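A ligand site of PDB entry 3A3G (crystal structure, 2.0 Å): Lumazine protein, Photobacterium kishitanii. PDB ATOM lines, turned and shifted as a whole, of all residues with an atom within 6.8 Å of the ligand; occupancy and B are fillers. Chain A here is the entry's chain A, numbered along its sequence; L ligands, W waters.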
ATOM      1  N   VAL A  41      -2.483 -17.830  33.529  1.00  0.00           N
ATOM      2  CA  VAL A  41      -3.693 -17.929  32.701  1.00  0.00           C
ATOM      3  C   VAL A  41      -4.182 -16.495  32.510  1.00  0.00           C
ATOM      4  O   VAL A  41      -4.501 -15.783  33.469  1.00  0.00           O
ATOM      5  CB  VAL A  41      -4.788 -18.860  33.341  1.00  0.00           C
ATOM      6  CG1 VAL A  41      -6.152 -18.763  32.580  1.00  0.00           C
ATOM      7  CG2 VAL A  41      -4.278 -20.292  33.430  1.00  0.00           C
ATOM      8  N   MET A  42      -4.203 -16.034  31.256  1.00  0.00           N
ATOM      9  CA  MET A  42      -4.560 -14.666  30.996  1.00  0.00           C
ATOM     10  C   MET A  42      -5.364 -14.678  29.710  1.00  0.00           C
ATOM     11  O   MET A  42      -5.523 -15.730  29.094  1.00  0.00           O
ATOM     12  CB  MET A  42      -3.271 -13.843  30.837  1.00  0.00           C
ATOM     13  CG  MET A  42      -2.390 -14.265  29.627  1.00  0.00           C
ATOM     14  SD  MET A  42      -0.995 -13.138  29.416  1.00  0.00           S
ATOM     15  CE  MET A  42      -1.847 -11.721  28.714  1.00  0.00           C
ATOM     16  N   GLY A  46      -9.179 -11.973  24.200  1.00  0.00           N
ATOM     17  CA  GLY A  46     -10.363 -12.392  24.983  1.00  0.00           C
ATOM     18  C   GLY A  46     -10.380 -13.864  25.338  1.00  0.00           C
ATOM     19  O   GLY A  46     -11.292 -14.334  26.015  1.00  0.00           O
ATOM     20  N   CYS A  47      -9.380 -14.617  24.863  1.00  0.00           N
ATOM     21  CA  CYS A  47      -9.407 -16.071  25.068  1.00  0.00           C
ATOM     22  C   CYS A  47      -8.469 -16.446  26.187  1.00  0.00           C
ATOM     23  O   CYS A  47      -7.279 -16.093  26.181  1.00  0.00           O
ATOM     24  CB  CYS A  47      -9.019 -16.818  23.763  1.00  0.00           C
ATOM     25  SG  CYS A  47      -9.075 -18.639  23.890  1.00  0.00           S
ATOM     26  N   SER A  48      -8.994 -17.178  27.157  1.00  0.00           N
ATOM     27  CA  SER A  48      -8.155 -17.727  28.240  1.00  0.00           C
ATOM     28  C   SER A  48      -7.153 -18.787  27.759  1.00  0.00           C
ATOM     29  O   SER A  48      -7.557 -19.834  27.187  1.00  0.00           O
ATOM     30  CB  SER A  48      -9.058 -18.289  29.339  1.00  0.00           C
ATOM     31  OG  SER A  48      -8.262 -18.753  30.380  1.00  0.00           O
ATOM     32  N   LEU A  49      -5.853 -18.521  27.978  1.00  0.00           N
ATOM     33  CA  LEU A  49      -4.759 -19.377  27.523  1.00  0.00           C
ATOM     34  C   LEU A  49      -3.701 -19.417  28.613  1.00  0.00           C
ATOM     35  O   LEU A  49      -3.632 -18.493  29.434  1.00  0.00           O
ATOM     36  CB  LEU A  49      -4.155 -18.844  26.207  1.00  0.00           C
ATOM     37  CG  LEU A  49      -5.045 -18.664  24.965  1.00  0.00           C
ATOM     38  CD1 LEU A  49      -4.199 -17.986  23.822  1.00  0.00           C
ATOM     39  CD2 LEU A  49      -5.660 -20.009  24.496  1.00  0.00           C
ATOM     40  N   THR A  50      -2.899 -20.488  28.619  1.00  0.00           N
ATOM     41  CA  THR A  50      -1.831 -20.677  29.620  1.00  0.00           C
ATOM     42  C   THR A  50      -0.462 -20.434  28.994  1.00  0.00           C
ATOM     43  O   THR A  50      -0.153 -21.060  27.987  1.00  0.00           O
ATOM     44  CB  THR A  50      -1.929 -22.129  30.153  1.00  0.00           C
ATOM     45  OG1 THR A  50      -3.282 -22.378  30.559  1.00  0.00           O
ATOM     46  CG2 THR A  50      -0.995 -22.395  31.391  1.00  0.00           C
ATOM     47  N   VAL A  51       0.338 -19.564  29.604  1.00  0.00           N
ATOM     48  CA  VAL A  51       1.729 -19.387  29.206  1.00  0.00           C
ATOM     49  C   VAL A  51       2.486 -20.708  29.373  1.00  0.00           C
ATOM     50  O   VAL A  51       2.505 -21.321  30.464  1.00  0.00           O
ATOM     51  CB  VAL A  51       2.454 -18.262  30.003  1.00  0.00           C
ATOM     52  CG1 VAL A  51       4.001 -18.151  29.617  1.00  0.00           C
ATOM     53  CG2 VAL A  51       1.737 -16.897  29.920  1.00  0.00           C
ATOM     54  N   VAL A  52       3.086 -21.152  28.276  1.00  0.00           N
ATOM     55  CA  VAL A  52       3.888 -22.381  28.197  1.00  0.00           C
ATOM     56  C   VAL A  52       5.408 -22.091  28.410  1.00  0.00           C
ATOM     57  O   VAL A  52       6.135 -22.891  29.016  1.00  0.00           O
ATOM     58  CB  VAL A  52       3.569 -23.082  26.852  1.00  0.00           C
ATOM     59  CG1 VAL A  52       4.634 -24.064  26.417  1.00  0.00           C
ATOM     60  CG2 VAL A  52       2.263 -23.817  26.994  1.00  0.00           C
ATOM     61  N   PHE A  61       2.167 -19.555  23.842  1.00  0.00           N
ATOM     62  CA  PHE A  61       0.949 -20.253  24.241  1.00  0.00           C
ATOM     63  C   PHE A  61       0.690 -21.376  23.276  1.00  0.00           C
ATOM     64  O   PHE A  61       0.939 -21.219  22.087  1.00  0.00           O
ATOM     65  CB  PHE A  61      -0.275 -19.322  24.197  1.00  0.00           C
ATOM     66  CG  PHE A  61      -0.169 -18.122  25.084  1.00  0.00           C
ATOM     67  CD1 PHE A  61      -0.759 -18.140  26.325  1.00  0.00           C
ATOM     68  CD2 PHE A  61       0.467 -16.972  24.665  1.00  0.00           C
ATOM     69  CE1 PHE A  61      -0.707 -17.021  27.181  1.00  0.00           C
ATOM     70  CE2 PHE A  61       0.540 -15.837  25.513  1.00  0.00           C
ATOM     71  CZ  PHE A  61      -0.056 -15.862  26.749  1.00  0.00           C
ATOM     72  N   ASP A  62       0.152 -22.489  23.775  1.00  0.00           N
ATOM     73  CA  ASP A  62      -0.363 -23.532  22.919  1.00  0.00           C
ATOM     74  C   ASP A  62      -1.857 -23.409  22.768  1.00  0.00           C
ATOM     75  O   ASP A  62      -2.586 -23.423  23.766  1.00  0.00           O
ATOM     76  CB  ASP A  62      -0.026 -24.915  23.485  1.00  0.00           C
ATOM     77  CG  ASP A  62       1.390 -25.294  23.233  1.00  0.00           C
ATOM     78  OD1 ASP A  62       1.922 -24.833  22.175  1.00  0.00           O
ATOM     79  OD2 ASP A  62       1.959 -26.036  24.051  1.00  0.00           O
ATOM     80  N   ILE A  63      -2.298 -23.289  21.522  1.00  0.00           N
ATOM     81  CA  ILE A  63      -3.714 -23.224  21.207  1.00  0.00           C
ATOM     82  C   ILE A  63      -4.102 -24.622  20.721  1.00  0.00           C
ATOM     83  O   ILE A  63      -3.667 -25.078  19.650  1.00  0.00           O
ATOM     84  CB  ILE A  63      -4.023 -22.152  20.147  1.00  0.00           C
ATOM     85  CG1 ILE A  63      -3.495 -20.768  20.636  1.00  0.00           C
ATOM     86  CG2 ILE A  63      -5.538 -22.089  19.884  1.00  0.00           C
ATOM     87  CD1 ILE A  63      -2.198 -20.425  20.011  1.00  0.00           C
ATOM     88  N   ASP A  64      -4.922 -25.263  21.520  1.00  0.00           N
ATOM     89  CA  ASP A  64      -5.330 -26.629  21.313  1.00  0.00           C
ATOM     90  C   ASP A  64      -6.821 -26.777  21.584  1.00  0.00           C
ATOM     91  O   ASP A  64      -7.648 -26.788  20.674  1.00  0.00           O
ATOM     92  CB  ASP A  64      -4.455 -27.602  22.149  1.00  0.00           C
ATOM     93  CG  ASP A  64      -4.270 -27.204  23.635  1.00  0.00           C
ATOM     94  OD1 ASP A  64      -5.232 -26.827  24.385  1.00  0.00           O
ATOM     95  OD2 ASP A  64      -3.117 -27.393  24.122  1.00  0.00           O
ATOM     96  N   GLN A  65      -7.184 -26.779  22.866  1.00  0.00           N
ATOM     97  CA  GLN A  65      -8.605 -26.768  23.258  1.00  0.00           C
ATOM     98  C   GLN A  65      -9.396 -25.673  22.555  1.00  0.00           C
ATOM     99  O   GLN A  65     -10.577 -25.872  22.158  1.00  0.00           O
ATOM    100  CB  GLN A  65      -8.709 -26.597  24.760  1.00  0.00           C
ATOM    101  CG  GLN A  65     -10.103 -26.859  25.245  1.00  0.00           C
ATOM    102  CD  GLN A  65     -10.258 -26.629  26.731  1.00  0.00           C
ATOM    103  OE1 GLN A  65      -9.293 -26.706  27.482  1.00  0.00           O
ATOM    104  NE2 GLN A  65     -11.495 -26.372  27.158  1.00  0.00           N
ATOM    105  N   ALA A  66      -8.764 -24.482  22.403  1.00  0.00           N
ATOM    106  CA  ALA A  66      -9.466 -23.325  21.803  1.00  0.00           C
ATOM    107  C   ALA A  66      -9.466 -23.297  20.269  1.00  0.00           C
ATOM    108  O   ALA A  66     -10.078 -22.398  19.671  1.00  0.00           O
ATOM    109  CB  ALA A  66      -8.816 -21.938  22.366  1.00  0.00           C
ATOM    110  N   ILE A  67      -8.748 -24.216  19.619  1.00  0.00           N
ATOM    111  CA  ILE A  67      -8.392 -24.028  18.206  1.00  0.00           C
ATOM    112  C   ILE A  67      -9.596 -23.959  17.238  1.00  0.00           C
ATOM    113  O   ILE A  67      -9.499 -23.339  16.153  1.00  0.00           O
ATOM    114  CB  ILE A  67      -7.371 -25.096  17.688  1.00  0.00           C
ATOM    115  CG1 ILE A  67      -6.761 -24.645  16.349  1.00  0.00           C
ATOM    116  CG2 ILE A  67      -8.057 -26.472  17.529  1.00  0.00           C
ATOM    117  CD1 ILE A  67      -5.344 -24.352  16.406  1.00  0.00           C
ATOM    118  N   ASN A  68     -10.731 -24.549  17.631  1.00  0.00           N
ATOM    119  CA  ASN A  68     -11.909 -24.651  16.739  1.00  0.00           C
ATOM    120  C   ASN A  68     -12.964 -23.564  16.890  1.00  0.00           C
ATOM    121  O   ASN A  68     -13.962 -23.511  16.107  1.00  0.00           O
ATOM    122  CB  ASN A  68     -12.580 -26.037  16.940  1.00  0.00           C
ATOM    123  CG  ASN A  68     -11.698 -27.162  16.500  1.00  0.00           C
ATOM    124  OD1 ASN A  68     -11.414 -28.059  17.292  1.00  0.00           O
ATOM    125  ND2 ASN A  68     -11.211 -27.091  15.283  1.00  0.00           N
ATOM    126  N   THR A  69     -12.773 -22.700  17.900  1.00  0.00           N
ATOM    127  CA  THR A  69     -13.783 -21.734  18.304  1.00  0.00           C
ATOM    128  C   THR A  69     -13.236 -20.311  18.432  1.00  0.00           C
ATOM    129  O   THR A  69     -13.903 -19.460  19.018  1.00  0.00           O
ATOM    130  CB  THR A  69     -14.440 -22.157  19.646  1.00  0.00           C
ATOM    131  OG1 THR A  69     -13.430 -22.438  20.636  1.00  0.00           O
ATOM    132  CG2 THR A  69     -15.265 -23.439  19.477  1.00  0.00           C
ATOM    133  N   THR A  70     -12.028 -20.085  17.902  1.00  0.00           N
ATOM    134  CA  THR A  70     -11.310 -18.802  18.016  1.00  0.00           C
ATOM    135  C   THR A  70     -10.613 -18.475  16.690  1.00  0.00           C
ATOM    136  O   THR A  70     -10.552 -19.312  15.781  1.00  0.00           O
ATOM    137  CB  THR A  70     -10.262 -18.803  19.130  1.00  0.00           C
ATOM    138  OG1 THR A  70      -9.275 -19.801  18.880  1.00  0.00           O
ATOM    139  CG2 THR A  70     -10.899 -19.020  20.529  1.00  0.00           C
ATOM    140  N   THR A  99     -15.072 -14.196  31.164  1.00  0.00           N
ATOM    141  CA  THR A  99     -14.508 -15.426  31.680  1.00  0.00           C
ATOM    142  C   THR A  99     -13.312 -15.872  30.835  1.00  0.00           C
ATOM    143  O   THR A  99     -12.445 -16.623  31.328  1.00  0.00           O
ATOM    144  CB  THR A  99     -15.536 -16.571  31.714  1.00  0.00           C
ATOM    145  OG1 THR A  99     -15.950 -16.830  30.372  1.00  0.00           O
ATOM    146  CG2 THR A  99     -16.727 -16.228  32.613  1.00  0.00           C
ATOM    147  N   GLY A 100     -13.245 -15.403  29.582  1.00  0.00           N
ATOM    148  CA  GLY A 100     -12.238 -15.904  28.629  1.00  0.00           C
ATOM    149  C   GLY A 100     -12.714 -17.171  27.915  1.00  0.00           C
ATOM    150  O   GLY A 100     -11.957 -17.811  27.184  1.00  0.00           O
ATOM    151  N   ASN A 101     -13.973 -17.538  28.132  1.00  0.00           N
ATOM    152  CA  ASN A 101     -14.563 -18.610  27.358  1.00  0.00           C
ATOM    153  C   ASN A 101     -15.168 -18.067  26.064  1.00  0.00           C
ATOM    154  O   ASN A 101     -16.262 -17.518  26.080  1.00  0.00           O
ATOM    155  CB  ASN A 101     -15.652 -19.369  28.121  1.00  0.00           C
ATOM    156  CG  ASN A 101     -16.019 -20.710  27.382  1.00  0.00           C
ATOM    157  OD1 ASN A 101     -15.163 -21.561  27.191  1.00  0.00           O
ATOM    158  ND2 ASN A 101     -17.243 -20.837  26.940  1.00  0.00           N
ATOM    159  N   ILE A 102     -14.461 -18.222  24.958  1.00  0.00           N
ATOM    160  CA  ILE A 102     -14.899 -17.656  23.664  1.00  0.00           C
ATOM    161  C   ILE A 102     -15.979 -18.584  23.081  1.00  0.00           C
ATOM    162  O   ILE A 102     -15.769 -19.794  22.950  1.00  0.00           O
ATOM    163  CB  ILE A 102     -13.767 -17.489  22.663  1.00  0.00           C
ATOM    164  CG1 ILE A 102     -12.696 -16.474  23.153  1.00  0.00           C
ATOM    165  CG2 ILE A 102     -14.311 -17.019  21.252  1.00  0.00           C
ATOM    166  CD1 ILE A 102     -13.299 -15.043  23.404  1.00  0.00           C
ATOM    167  N   LYS A 103     -17.134 -17.997  22.786  1.00  0.00           N
ATOM    168  CA  LYS A 103     -18.308 -18.759  22.365  1.00  0.00           C
ATOM    169  C   LYS A 103     -18.131 -19.119  20.925  1.00  0.00           C
ATOM    170  O   LYS A 103     -18.568 -20.196  20.491  1.00  0.00           O
ATOM    171  CB  LYS A 103     -19.579 -17.929  22.542  1.00  0.00           C
ATOM    172  CG  LYS A 103     -19.722 -17.381  23.929  1.00  0.00           C
ATOM    173  CD  LYS A 103     -19.686 -18.484  25.036  1.00  0.00           C
ATOM    174  CE  LYS A 103     -19.928 -17.853  26.397  1.00  0.00           C
ATOM    175  NZ  LYS A 103     -19.219 -18.511  27.531  1.00  0.00           N
ATOM    176  N   GLY A 104     -17.463 -18.244  20.180  1.00  0.00           N
ATOM    177  CA  GLY A 104     -17.162 -18.563  18.800  1.00  0.00           C
ATOM    178  C   GLY A 104     -16.678 -17.388  18.010  1.00  0.00           C
ATOM    179  O   GLY A 104     -16.518 -16.302  18.552  1.00  0.00           O
HETATM  180  C1  LIG L   1      -9.351 -22.354  29.791  1.00  0.00           C
HETATM  181  C2  LIG L   1      -8.190 -22.488  29.015  1.00  0.00           C
HETATM  182  C3  LIG L   1      -6.952 -22.313  29.643  1.00  0.00           C
HETATM  183  C4  LIG L   1      -6.890 -21.960  31.001  1.00  0.00           C
HETATM  184  N1  LIG L   1      -5.781 -22.501  28.885  1.00  0.00           N
HETATM  185  C5  LIG L   1      -5.826 -22.821  27.497  1.00  0.00           C
HETATM  186  C6  LIG L   1      -4.685 -22.947  26.666  1.00  0.00           C
HETATM  187  O1  LIG L   1      -3.529 -22.788  27.044  1.00  0.00           O
HETATM  188  N2  LIG L   1      -4.830 -23.307  25.344  1.00  0.00           N
HETATM  189  C7  LIG L   1      -6.083 -23.512  24.806  1.00  0.00           C
HETATM  190  O2  LIG L   1      -6.221 -23.825  23.632  1.00  0.00           O
HETATM  191  N3  LIG L   1      -7.180 -23.349  25.586  1.00  0.00           N
HETATM  192  C8  LIG L   1      -7.076 -22.996  26.909  1.00  0.00           C
HETATM  193  N4  LIG L   1      -8.242 -22.876  27.645  1.00  0.00           N
HETATM  194  C9  LIG L   1      -9.514 -23.107  26.922  1.00  0.00           C
HETATM  195  C10 LIG L   1      -9.959 -21.915  26.039  1.00  0.00           C
HETATM  196  O3  LIG L   1     -10.091 -20.706  26.816  1.00  0.00           O
HETATM  197  C11 LIG L   1     -11.324 -22.251  25.466  1.00  0.00           C
HETATM  198  O4  LIG L   1     -11.142 -23.466  24.761  1.00  0.00           O
HETATM  199  C12 LIG L   1     -11.860 -21.216  24.487  1.00  0.00           C
HETATM  200  O5  LIG L   1     -12.183 -19.968  25.114  1.00  0.00           O
HETATM  201  C13 LIG L   1     -13.123 -21.749  23.808  1.00  0.00           C
HETATM  202  O6  LIG L   1     -13.346 -20.888  22.688  1.00  0.00           O
HETATM  203  O   HOH W   1      -0.906 -22.813  26.442  1.00  0.00           O
HETATM  204  O   HOH W   2     -12.266 -20.780  28.716  1.00  0.00           O
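The backbone carbonyl oxygen (O) of Ala 66 is in hydrogen-bond range of the side-chain hydroxyl (OG1) of Thr 69.
The backbone carbonyl oxygen (O) of Gly 100 lies within hydrogen-bond range of the backbone NH (N) of Ser 48.
O of Ala 66 lies within hydrogen-bond range of OG1 of Thr 70 (2.8 Å).
N of Leu 49 is in hydrogen-bond range of O of Met 42.
The side-chain amide nitrogen (ND2) of Asn 101 sits close to the side-chain amino group (NZ) of Lys 103 (3.1 Å).
The backbone NH (N) of Asn 101 is in hydrogen-bond range of the side-chain hydroxyl (OG1) of Thr 99.
Merely in contact with the ligand: Leu 49 (3.5 Å), Ile 63 (3.5 Å), Asn 101 (3.5 Å), Val 41 (3.6 Å) and Thr 70 (3.8 Å).
Hydrophobic or aromatic side chains that line the ligand: Val 41, Leu 49, Ala 66 and Ile 102.
Within 4 Å of the ligand: Val 41, Cys 47, Ser 48, Leu 49, Thr 50, Asp 62, Ile 63, Asp 64, Gln 65, Ala 66, Thr 69, Thr 70, Gly 100, Asn 101 and Ile 102.
Water W1 lies within hydrogen-bond range of the backbone carbonyl oxygen of Thr 50, an oxygen (O1) of the ligand and the backbone NH of Asp 62.
Water W2 lies within hydrogen-bond range of O3 of the ligand (2.9 Å), O of Gly 100 (3.4 Å) and OD1 of Asn 101 (3.4 Å).
O6 of the ligand is in hydrogen-bond range of OG1 of Thr 69.
The backbone NH (N) of Ile 102 sits at hydrogen-bond distance from an oxygen (O5) of the ligand (2.9 Å).
An oxygen (O6) of the ligand lies within hydrogen-bond range of the backbone carbonyl oxygen (O) of Ile 102 (2.7 Å).
The backbone carbonyl oxygen (O) of Ser 48 lies within hydrogen-bond range of an oxygen (O3) of the ligand, at 2.7 Å.
The backbone carbonyl oxygen (O) of Asp 62 is in hydrogen-bond range of a nitrogen (N2) of the ligand (2.7 Å).
The backbone NH (N) of Thr 50 sits at hydrogen-bond distance from an oxygen (O1) of the ligand (2.9 Å).
The side-chain hydroxyl of Thr 50 is in hydrogen-bond range of a nitrogen (N1) of the ligand (3.0 Å).
O2 of the ligand sits at hydrogen-bond distance from N of Asp 64, at 2.9 Å.
The backbone NH of Ala 66 sits at hydrogen-bond distance from an oxygen (O2) of the ligand (2.9 Å).
O of Gly 100 sits at hydrogen-bond distance from O5 of the ligand, at 3.0 Å.
O2 of the ligand is in hydrogen-bond range of N of Gln 65 (3.2 Å).
SG of Cys 47 lies within hydrogen-bond range of O5 of the ligand (3.6 Å).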
